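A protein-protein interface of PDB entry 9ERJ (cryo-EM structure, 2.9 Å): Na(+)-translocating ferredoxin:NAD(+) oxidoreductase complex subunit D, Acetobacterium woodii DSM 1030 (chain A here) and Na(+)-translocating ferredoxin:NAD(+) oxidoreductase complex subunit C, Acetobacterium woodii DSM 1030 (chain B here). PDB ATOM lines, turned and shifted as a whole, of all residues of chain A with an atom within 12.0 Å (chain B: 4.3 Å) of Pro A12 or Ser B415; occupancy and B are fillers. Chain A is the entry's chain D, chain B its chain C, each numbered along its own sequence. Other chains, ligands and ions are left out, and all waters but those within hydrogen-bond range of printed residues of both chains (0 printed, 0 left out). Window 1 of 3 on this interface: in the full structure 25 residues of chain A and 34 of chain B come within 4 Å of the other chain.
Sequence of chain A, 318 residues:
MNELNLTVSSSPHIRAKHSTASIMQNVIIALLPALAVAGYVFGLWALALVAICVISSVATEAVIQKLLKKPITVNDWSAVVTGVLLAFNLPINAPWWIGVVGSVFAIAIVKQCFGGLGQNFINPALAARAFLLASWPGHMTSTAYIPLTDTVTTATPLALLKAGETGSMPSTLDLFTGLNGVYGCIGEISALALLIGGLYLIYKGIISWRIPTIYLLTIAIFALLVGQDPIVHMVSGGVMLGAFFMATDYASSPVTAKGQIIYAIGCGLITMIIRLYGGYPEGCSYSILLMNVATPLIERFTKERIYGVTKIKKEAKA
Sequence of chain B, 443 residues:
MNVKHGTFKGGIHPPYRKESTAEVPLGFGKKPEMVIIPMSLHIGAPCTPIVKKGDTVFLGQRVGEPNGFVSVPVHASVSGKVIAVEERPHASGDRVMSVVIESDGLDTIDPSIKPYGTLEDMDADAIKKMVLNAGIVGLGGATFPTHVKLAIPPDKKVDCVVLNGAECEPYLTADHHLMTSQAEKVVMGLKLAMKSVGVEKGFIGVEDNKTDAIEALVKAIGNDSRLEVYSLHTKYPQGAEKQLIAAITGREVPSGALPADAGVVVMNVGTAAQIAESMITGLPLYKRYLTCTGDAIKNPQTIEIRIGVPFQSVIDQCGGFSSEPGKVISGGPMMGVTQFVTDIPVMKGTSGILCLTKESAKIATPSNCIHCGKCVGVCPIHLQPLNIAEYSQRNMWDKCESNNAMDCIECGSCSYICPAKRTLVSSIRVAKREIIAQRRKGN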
ATOM      1  N   THR A   7      -5.482   5.303  17.282  1.00  0.00           N
ATOM      2  CA  THR A   7      -5.813   4.217  18.193  1.00  0.00           C
ATOM      3  C   THR A   7      -5.234   2.909  17.670  1.00  0.00           C
ATOM      4  O   THR A   7      -5.317   2.617  16.474  1.00  0.00           O
ATOM      5  CB  THR A   7      -7.328   4.085  18.361  1.00  0.00           C
ATOM      6  OG1 THR A   7      -7.899   5.379  18.585  1.00  0.00           O
ATOM      7  CG2 THR A   7      -7.664   3.185  19.537  1.00  0.00           C
ATOM      8  N   VAL A   8      -4.643   2.128  18.570  1.00  0.00           N
ATOM      9  CA  VAL A   8      -4.052   0.839  18.234  1.00  0.00           C
ATOM     10  C   VAL A   8      -4.798  -0.247  18.997  1.00  0.00           C
ATOM     11  O   VAL A   8      -5.063  -0.102  20.196  1.00  0.00           O
ATOM     12  CB  VAL A   8      -2.543   0.799  18.545  1.00  0.00           C
ATOM     13  CG1 VAL A   8      -1.766   1.531  17.468  1.00  0.00           C
ATOM     14  CG2 VAL A   8      -2.252   1.403  19.907  1.00  0.00           C
ATOM     15  N   SER A   9      -5.149  -1.321  18.297  1.00  0.00           N
ATOM     16  CA  SER A   9      -5.868  -2.439  18.891  1.00  0.00           C
ATOM     17  C   SER A   9      -5.641  -3.666  18.018  1.00  0.00           C
ATOM     18  O   SER A   9      -4.802  -3.664  17.114  1.00  0.00           O
ATOM     19  CB  SER A   9      -7.358  -2.125  19.042  1.00  0.00           C
ATOM     20  OG  SER A   9      -7.892  -1.601  17.840  1.00  0.00           O
ATOM     21  N   SER A  10      -6.400  -4.718  18.297  1.00  0.00           N
ATOM     22  CA  SER A  10      -6.329  -5.958  17.543  1.00  0.00           C
ATOM     23  C   SER A  10      -7.570  -6.127  16.674  1.00  0.00           C
ATOM     24  O   SER A  10      -8.599  -5.478  16.880  1.00  0.00           O
ATOM     25  CB  SER A  10      -6.176  -7.155  18.486  1.00  0.00           C
ATOM     26  OG  SER A  10      -6.402  -8.374  17.805  1.00  0.00           O
ATOM     27  N   SER A  11      -7.455  -7.012  15.688  1.00  0.00           N
ATOM     28  CA  SER A  11      -8.551  -7.266  14.768  1.00  0.00           C
ATOM     29  C   SER A  11      -9.686  -8.000  15.483  1.00  0.00           C
ATOM     30  O   SER A  11      -9.452  -8.701  16.471  1.00  0.00           O
ATOM     31  CB  SER A  11      -8.054  -8.092  13.585  1.00  0.00           C
ATOM     32  OG  SER A  11      -6.963  -7.453  12.950  1.00  0.00           O
ATOM     33  N   PRO A  12     -10.936  -7.857  15.008  1.00  0.00           N
ATOM     34  CA  PRO A  12     -11.433  -7.036  13.891  1.00  0.00           C
ATOM     35  C   PRO A  12     -11.602  -5.569  14.262  1.00  0.00           C
ATOM     36  O   PRO A  12     -11.513  -5.198  15.427  1.00  0.00           O
ATOM     37  CB  PRO A  12     -12.793  -7.679  13.558  1.00  0.00           C
ATOM     38  CG  PRO A  12     -12.858  -8.960  14.351  1.00  0.00           C
ATOM     39  CD  PRO A  12     -12.012  -8.698  15.549  1.00  0.00           C
ATOM     40  N   HIS A  13     -11.853  -4.708  13.277  1.00  0.00           N
ATOM     41  CA  HIS A  13     -12.088  -3.293  13.519  1.00  0.00           C
ATOM     42  C   HIS A  13     -13.534  -2.888  13.257  1.00  0.00           C
ATOM     43  O   HIS A  13     -13.850  -1.695  13.301  1.00  0.00           O
ATOM     44  CB  HIS A  13     -11.133  -2.451  12.670  1.00  0.00           C
ATOM     45  CG  HIS A  13      -9.701  -2.883  12.765  1.00  0.00           C
ATOM     46  ND1 HIS A  13      -8.922  -2.640  13.875  1.00  0.00           N
ATOM     47  CD2 HIS A  13      -8.911  -3.548  11.890  1.00  0.00           C
ATOM     48  CE1 HIS A  13      -7.713  -3.133  13.679  1.00  0.00           C
ATOM     49  NE2 HIS A  13      -7.680  -3.691  12.483  1.00  0.00           N
ATOM     50  N   ILE A  14     -14.416  -3.850  12.985  1.00  0.00           N
ATOM     51  CA  ILE A  14     -15.840  -3.599  12.805  1.00  0.00           C
ATOM     52  C   ILE A  14     -16.620  -4.639  13.598  1.00  0.00           C
ATOM     53  O   ILE A  14     -16.147  -5.757  13.822  1.00  0.00           O
ATOM     54  CB  ILE A  14     -16.257  -3.629  11.317  1.00  0.00           C
ATOM     55  CG1 ILE A  14     -15.749  -4.903  10.642  1.00  0.00           C
ATOM     56  CG2 ILE A  14     -15.747  -2.397  10.591  1.00  0.00           C
ATOM     57  CD1 ILE A  14     -16.376  -5.167   9.294  1.00  0.00           C
ATOM     58  N   ARG A  15     -17.826  -4.265  14.024  1.00  0.00           N
ATOM     59  CA  ARG A  15     -18.689  -5.127  14.822  1.00  0.00           C
ATOM     60  C   ARG A  15     -20.107  -5.085  14.265  1.00  0.00           C
ATOM     61  O   ARG A  15     -20.410  -4.343  13.327  1.00  0.00           O
ATOM     62  CB  ARG A  15     -18.686  -4.713  16.301  1.00  0.00           C
ATOM     63  CG  ARG A  15     -17.319  -4.694  16.960  1.00  0.00           C
ATOM     64  CD  ARG A  15     -17.004  -6.021  17.627  1.00  0.00           C
ATOM     65  NE  ARG A  15     -15.788  -5.964  18.431  1.00  0.00           N
ATOM     66  CZ  ARG A  15     -14.558  -5.966  17.938  1.00  0.00           C
ATOM     67  NH1 ARG A  15     -14.333  -6.022  16.637  1.00  0.00           N
ATOM     68  NH2 ARG A  15     -13.525  -5.915  18.774  1.00  0.00           N
ATOM     69  N   ALA A  16     -20.982  -5.896  14.853  1.00  0.00           N
ATOM     70  CA  ALA A  16     -22.389  -5.930  14.488  1.00  0.00           C
ATOM     71  C   ALA A  16     -23.158  -4.841  15.234  1.00  0.00           C
ATOM     72  O   ALA A  16     -22.586  -4.016  15.948  1.00  0.00           O
ATOM     73  CB  ALA A  16     -22.984  -7.306  14.778  1.00  0.00           C
ATOM     74  N   LYS A  17     -24.479  -4.843  15.057  1.00  0.00           N
ATOM     75  CA  LYS A  17     -25.317  -3.814  15.662  1.00  0.00           C
ATOM     76  C   LYS A  17     -26.026  -4.277  16.927  1.00  0.00           C
ATOM     77  O   LYS A  17     -26.270  -3.461  17.821  1.00  0.00           O
ATOM     78  CB  LYS A  17     -26.357  -3.321  14.652  1.00  0.00           C
ATOM     79  CG  LYS A  17     -25.776  -2.492  13.521  1.00  0.00           C
ATOM     80  CD  LYS A  17     -24.998  -1.302  14.055  1.00  0.00           C
ATOM     81  CE  LYS A  17     -23.712  -1.088  13.272  1.00  0.00           C
ATOM     82  NZ  LYS A  17     -22.660  -0.430  14.095  1.00  0.00           N
ATOM     83  N   HIS A  18     -26.365  -5.560  17.027  1.00  0.00           N
ATOM     84  CA  HIS A  18     -27.103  -6.050  18.182  1.00  0.00           C
ATOM     85  C   HIS A  18     -26.212  -6.108  19.418  1.00  0.00           C
ATOM     86  O   HIS A  18     -24.994  -6.280  19.329  1.00  0.00           O
ATOM     87  CB  HIS A  18     -27.695  -7.430  17.893  1.00  0.00           C
ATOM     88  CG  HIS A  18     -26.672  -8.510  17.726  1.00  0.00           C
ATOM     89  ND1 HIS A  18     -26.074  -8.787  16.517  1.00  0.00           N
ATOM     90  CD2 HIS A  18     -26.145  -9.384  18.615  1.00  0.00           C
ATOM     91  CE1 HIS A  18     -25.221  -9.785  16.668  1.00  0.00           C
ATOM     92  NE2 HIS A  18     -25.245 -10.165  17.932  1.00  0.00           N
ATOM     93  N   SER A  19     -26.839  -5.959  20.584  1.00  0.00           N
ATOM     94  CA  SER A  19     -26.138  -5.977  21.861  1.00  0.00           C
ATOM     95  C   SER A  19     -26.994  -6.738  22.868  1.00  0.00           C
ATOM     96  O   SER A  19     -27.974  -7.396  22.510  1.00  0.00           O
ATOM     97  CB  SER A  19     -25.818  -4.550  22.323  1.00  0.00           C
ATOM     98  OG  SER A  19     -26.992  -3.762  22.400  1.00  0.00           O
ATOM     99  N   PRO B 333     -10.495  -4.303   6.822  1.00  0.00           N
ATOM    100  CA  PRO B 333     -11.046  -4.032   8.156  1.00  0.00           C
ATOM    101  C   PRO B 333     -11.143  -5.256   9.050  1.00  0.00           C
ATOM    102  O   PRO B 333     -11.437  -5.103  10.242  1.00  0.00           O
ATOM    103  CB  PRO B 333     -12.440  -3.475   7.846  1.00  0.00           C
ATOM    104  CG  PRO B 333     -12.806  -4.098   6.549  1.00  0.00           C
ATOM    105  CD  PRO B 333     -11.528  -4.269   5.774  1.00  0.00           C
ATOM    106  N   MET B 334     -10.907  -6.457   8.522  1.00  0.00           N
ATOM    107  CA  MET B 334     -11.091  -7.681   9.288  1.00  0.00           C
ATOM    108  C   MET B 334      -9.785  -8.360   9.676  1.00  0.00           C
ATOM    109  O   MET B 334      -9.777  -9.146  10.627  1.00  0.00           O
ATOM    110  CB  MET B 334     -11.956  -8.667   8.495  1.00  0.00           C
ATOM    111  CG  MET B 334     -13.419  -8.648   8.895  1.00  0.00           C
ATOM    112  SD  MET B 334     -13.691  -9.384  10.513  1.00  0.00           S
ATOM    113  CE  MET B 334     -15.419  -9.798  10.397  1.00  0.00           C
ATOM    114  N   GLY B 412     -11.410 -13.714  12.783  1.00  0.00           N
ATOM    115  CA  GLY B 412     -12.166 -12.561  13.231  1.00  0.00           C
ATOM    116  C   GLY B 412     -13.638 -12.792  13.514  1.00  0.00           C
ATOM    117  O   GLY B 412     -14.176 -12.206  14.456  1.00  0.00           O
ATOM    118  N   SER B 413     -14.300 -13.596  12.673  1.00  0.00           N
ATOM    119  CA  SER B 413     -15.743 -13.850  12.696  1.00  0.00           C
ATOM    120  C   SER B 413     -16.344 -14.030  14.087  1.00  0.00           C
ATOM    121  O   SER B 413     -17.413 -13.482  14.376  1.00  0.00           O
ATOM    122  CB  SER B 413     -16.072 -15.087  11.857  1.00  0.00           C
ATOM    123  OG  SER B 413     -15.292 -15.137  10.677  1.00  0.00           O
ATOM    124  N   CYS B 414     -15.680 -14.807  14.947  1.00  0.00           N
ATOM    125  CA  CYS B 414     -16.219 -15.072  16.279  1.00  0.00           C
ATOM    126  C   CYS B 414     -16.285 -13.804  17.123  1.00  0.00           C
ATOM    127  O   CYS B 414     -17.214 -13.630  17.920  1.00  0.00           O
ATOM    128  CB  CYS B 414     -15.384 -16.146  16.977  1.00  0.00           C
ATOM    129  SG  CYS B 414     -13.674 -15.687  17.320  1.00  0.00           S
ATOM    130  N   SER B 415     -15.310 -12.908  16.967  1.00  0.00           N
ATOM    131  CA  SER B 415     -15.305 -11.658  17.715  1.00  0.00           C
ATOM    132  C   SER B 415     -16.240 -10.611  17.124  1.00  0.00           C
ATOM    133  O   SER B 415     -16.576  -9.640  17.809  1.00  0.00           O
ATOM    134  CB  SER B 415     -13.884 -11.095  17.783  1.00  0.00           C
ATOM    135  OG  SER B 415     -13.735 -10.215  18.879  1.00  0.00           O
ATOM    136  N   TYR B 416     -16.659 -10.785  15.870  1.00  0.00           N
ATOM    137  CA  TYR B 416     -17.528  -9.823  15.202  1.00  0.00           C
ATOM    138  C   TYR B 416     -18.980  -9.948  15.647  1.00  0.00           C
ATOM    139  O   TYR B 416     -19.700  -8.945  15.685  1.00  0.00           O
ATOM    140  CB  TYR B 416     -17.404 -10.005  13.686  1.00  0.00           C
ATOM    141  CG  TYR B 416     -18.436  -9.297  12.834  1.00  0.00           C
ATOM    142  CD1 TYR B 416     -18.229  -7.994  12.403  1.00  0.00           C
ATOM    143  CD2 TYR B 416     -19.592  -9.944  12.420  1.00  0.00           C
ATOM    144  CE1 TYR B 416     -19.158  -7.348  11.613  1.00  0.00           C
ATOM    145  CE2 TYR B 416     -20.526  -9.304  11.630  1.00  0.00           C
ATOM    146  CZ  TYR B 416     -20.303  -8.009  11.230  1.00  0.00           C
ATOM    147  OH  TYR B 416     -21.229  -7.368  10.444  1.00  0.00           O
ATOM    148  N   ILE B 417     -19.427 -11.161  15.994  1.00  0.00           N
ATOM    149  CA  ILE B 417     -20.840 -11.422  16.252  1.00  0.00           C
ATOM    150  C   ILE B 417     -21.200 -11.352  17.733  1.00  0.00           C
ATOM    151  O   ILE B 417     -22.383 -11.476  18.079  1.00  0.00           O
ATOM    152  CB  ILE B 417     -21.224 -12.798  15.662  1.00  0.00           C
ATOM    153  CG1 ILE B 417     -22.697 -12.833  15.246  1.00  0.00           C
ATOM    154  CG2 ILE B 417     -20.896 -13.919  16.636  1.00  0.00           C
ATOM    155  CD1 ILE B 417     -22.980 -12.141  13.938  1.00  0.00           C
ATOM    156  N   CYS B 418     -20.232 -11.132  18.611  1.00  0.00           N
ATOM    157  CA  CYS B 418     -20.474 -11.204  20.051  1.00  0.00           C
ATOM    158  C   CYS B 418     -21.351 -10.051  20.526  1.00  0.00           C
ATOM    159  O   CYS B 418     -20.996  -8.886  20.309  1.00  0.00           O
ATOM    160  CB  CYS B 418     -19.145 -11.191  20.799  1.00  0.00           C
ATOM    161  SG  CYS B 418     -19.230 -11.807  22.488  1.00  0.00           S
ATOM    162  N   ARG B 422     -16.614  -8.746  23.101  1.00  0.00           N
ATOM    163  CA  ARG B 422     -15.418  -9.294  23.717  1.00  0.00           C
ATOM    164  C   ARG B 422     -14.302  -9.453  22.686  1.00  0.00           C
ATOM    165  O   ARG B 422     -14.463  -9.170  21.497  1.00  0.00           O
ATOM    166  CB  ARG B 422     -15.730 -10.623  24.406  1.00  0.00           C
ATOM    167  CG  ARG B 422     -17.058 -10.638  25.134  1.00  0.00           C
ATOM    168  CD  ARG B 422     -17.188 -11.850  26.035  1.00  0.00           C
ATOM    169  NE  ARG B 422     -16.651 -11.592  27.365  1.00  0.00           N
ATOM    170  CZ  ARG B 422     -15.881 -12.434  28.038  1.00  0.00           C
ATOM    171  NH1 ARG B 422     -15.544 -13.613  27.539  1.00  0.00           N
ATOM    172  NH2 ARG B 422     -15.436 -12.085  29.242  1.00  0.00           N
ATOM    173  N   THR B 423     -13.151  -9.930  23.161  1.00  0.00           N
ATOM    174  CA  THR B 423     -11.911  -9.968  22.393  1.00  0.00           C
ATOM    175  C   THR B 423     -11.403 -11.398  22.242  1.00  0.00           C
ATOM    176  O   THR B 423     -10.250 -11.684  22.574  1.00  0.00           O
ATOM    177  CB  THR B 423     -10.838  -9.100  23.053  1.00  0.00           C
ATOM    178  OG1 THR B 423     -10.457  -9.679  24.305  1.00  0.00           O
ATOM    179  CG2 THR B 423     -11.355  -7.689  23.288  1.00  0.00           C
ATOM    180  N   LEU B 424     -12.274 -12.298  21.775  1.00  0.00           N
ATOM    181  CA  LEU B 424     -11.989 -13.732  21.803  1.00  0.00           C
ATOM    182  C   LEU B 424     -10.746 -14.092  20.993  1.00  0.00           C
ATOM    183  O   LEU B 424      -9.923 -14.907  21.436  1.00  0.00           O
ATOM    184  CB  LEU B 424     -13.203 -14.502  21.285  1.00  0.00           C
ATOM    185  CG  LEU B 424     -14.560 -14.095  21.865  1.00  0.00           C
ATOM    186  CD1 LEU B 424     -15.687 -14.814  21.155  1.00  0.00           C
ATOM    187  CD2 LEU B 424     -14.606 -14.381  23.351  1.00  0.00           C
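N of His A13 lies within hydrogen-bond range of O of Pro B333 (3.1 Å).
O of Tyr B416 lies within hydrogen-bond range of N of Ala A16 (3.4 Å).
NE2 of His A18 sits at hydrogen-bond distance from O of Ile B417, at 3.2 Å.
The side-chain hydroxyl of Ser B415 sits at hydrogen-bond distance from the backbone carbonyl oxygen of Arg B422, at 2.9 Å.
The backbone carbonyl oxygen (O) of Pro A12 lies within hydrogen-bond range of the guanidinium group (NH1) of Arg A15, at 3.2 Å.
Among the printed residues, pairs that only touch across the chains: Ser A11 with Met B334, Pro A12 with Met B334, Pro A12 with Gly B412, Pro A12 with Ser B415, Ile A14 with Tyr B416, Arg A15 with Ser B415 and Arg A15 with Tyr B416.
Pro A12 touches just these residues of chain B: Met B334 (3.6 Å), Gly B412 (3.5 Å) and Ser B415 (3.8 Å).
Met B334 touches two residues of chain A.
Of chain A, only Pro A12 comes within 4 Å of Gly B412.
No residue of chain A comes within 4 Å of Cys B414.
Ile B417 touches one residue of chain A.
No residue of chain A comes within 4 Å of Cys B418.
No residue of chain A comes within 4 Å of Thr B423.
Leu B424 touches none of the printed residues of chain A.
Printed residues of chain B within 4 Å of Ile A14: Tyr B416 (3.4 Å).
Of the printed residues of chain A, Tyr B416 touches Ile A14, Arg A15 and Ala A16.
Of the printed residues of chain B, His A13 touches Pro B333.
Printed residues of chain B within 4 Å of Ala A16: Tyr B416.
The nearest residue of chain A that does not touch Ser B415 is Ser A11 (5.1 Å).
Of the 12 printed residues of chain B, 6 touch a printed residue of chain A.
Along chain B the printed residues that touch a printed residue of chain A span positions 333 to 417.
Of the 13 printed residues of chain A, 7 touch a printed residue of chain B.
Hydrophobic or aromatic side chains of chain A within 4 Å of the printed part of chain B: Pro A12, His A13, Ala A16 and His A18.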
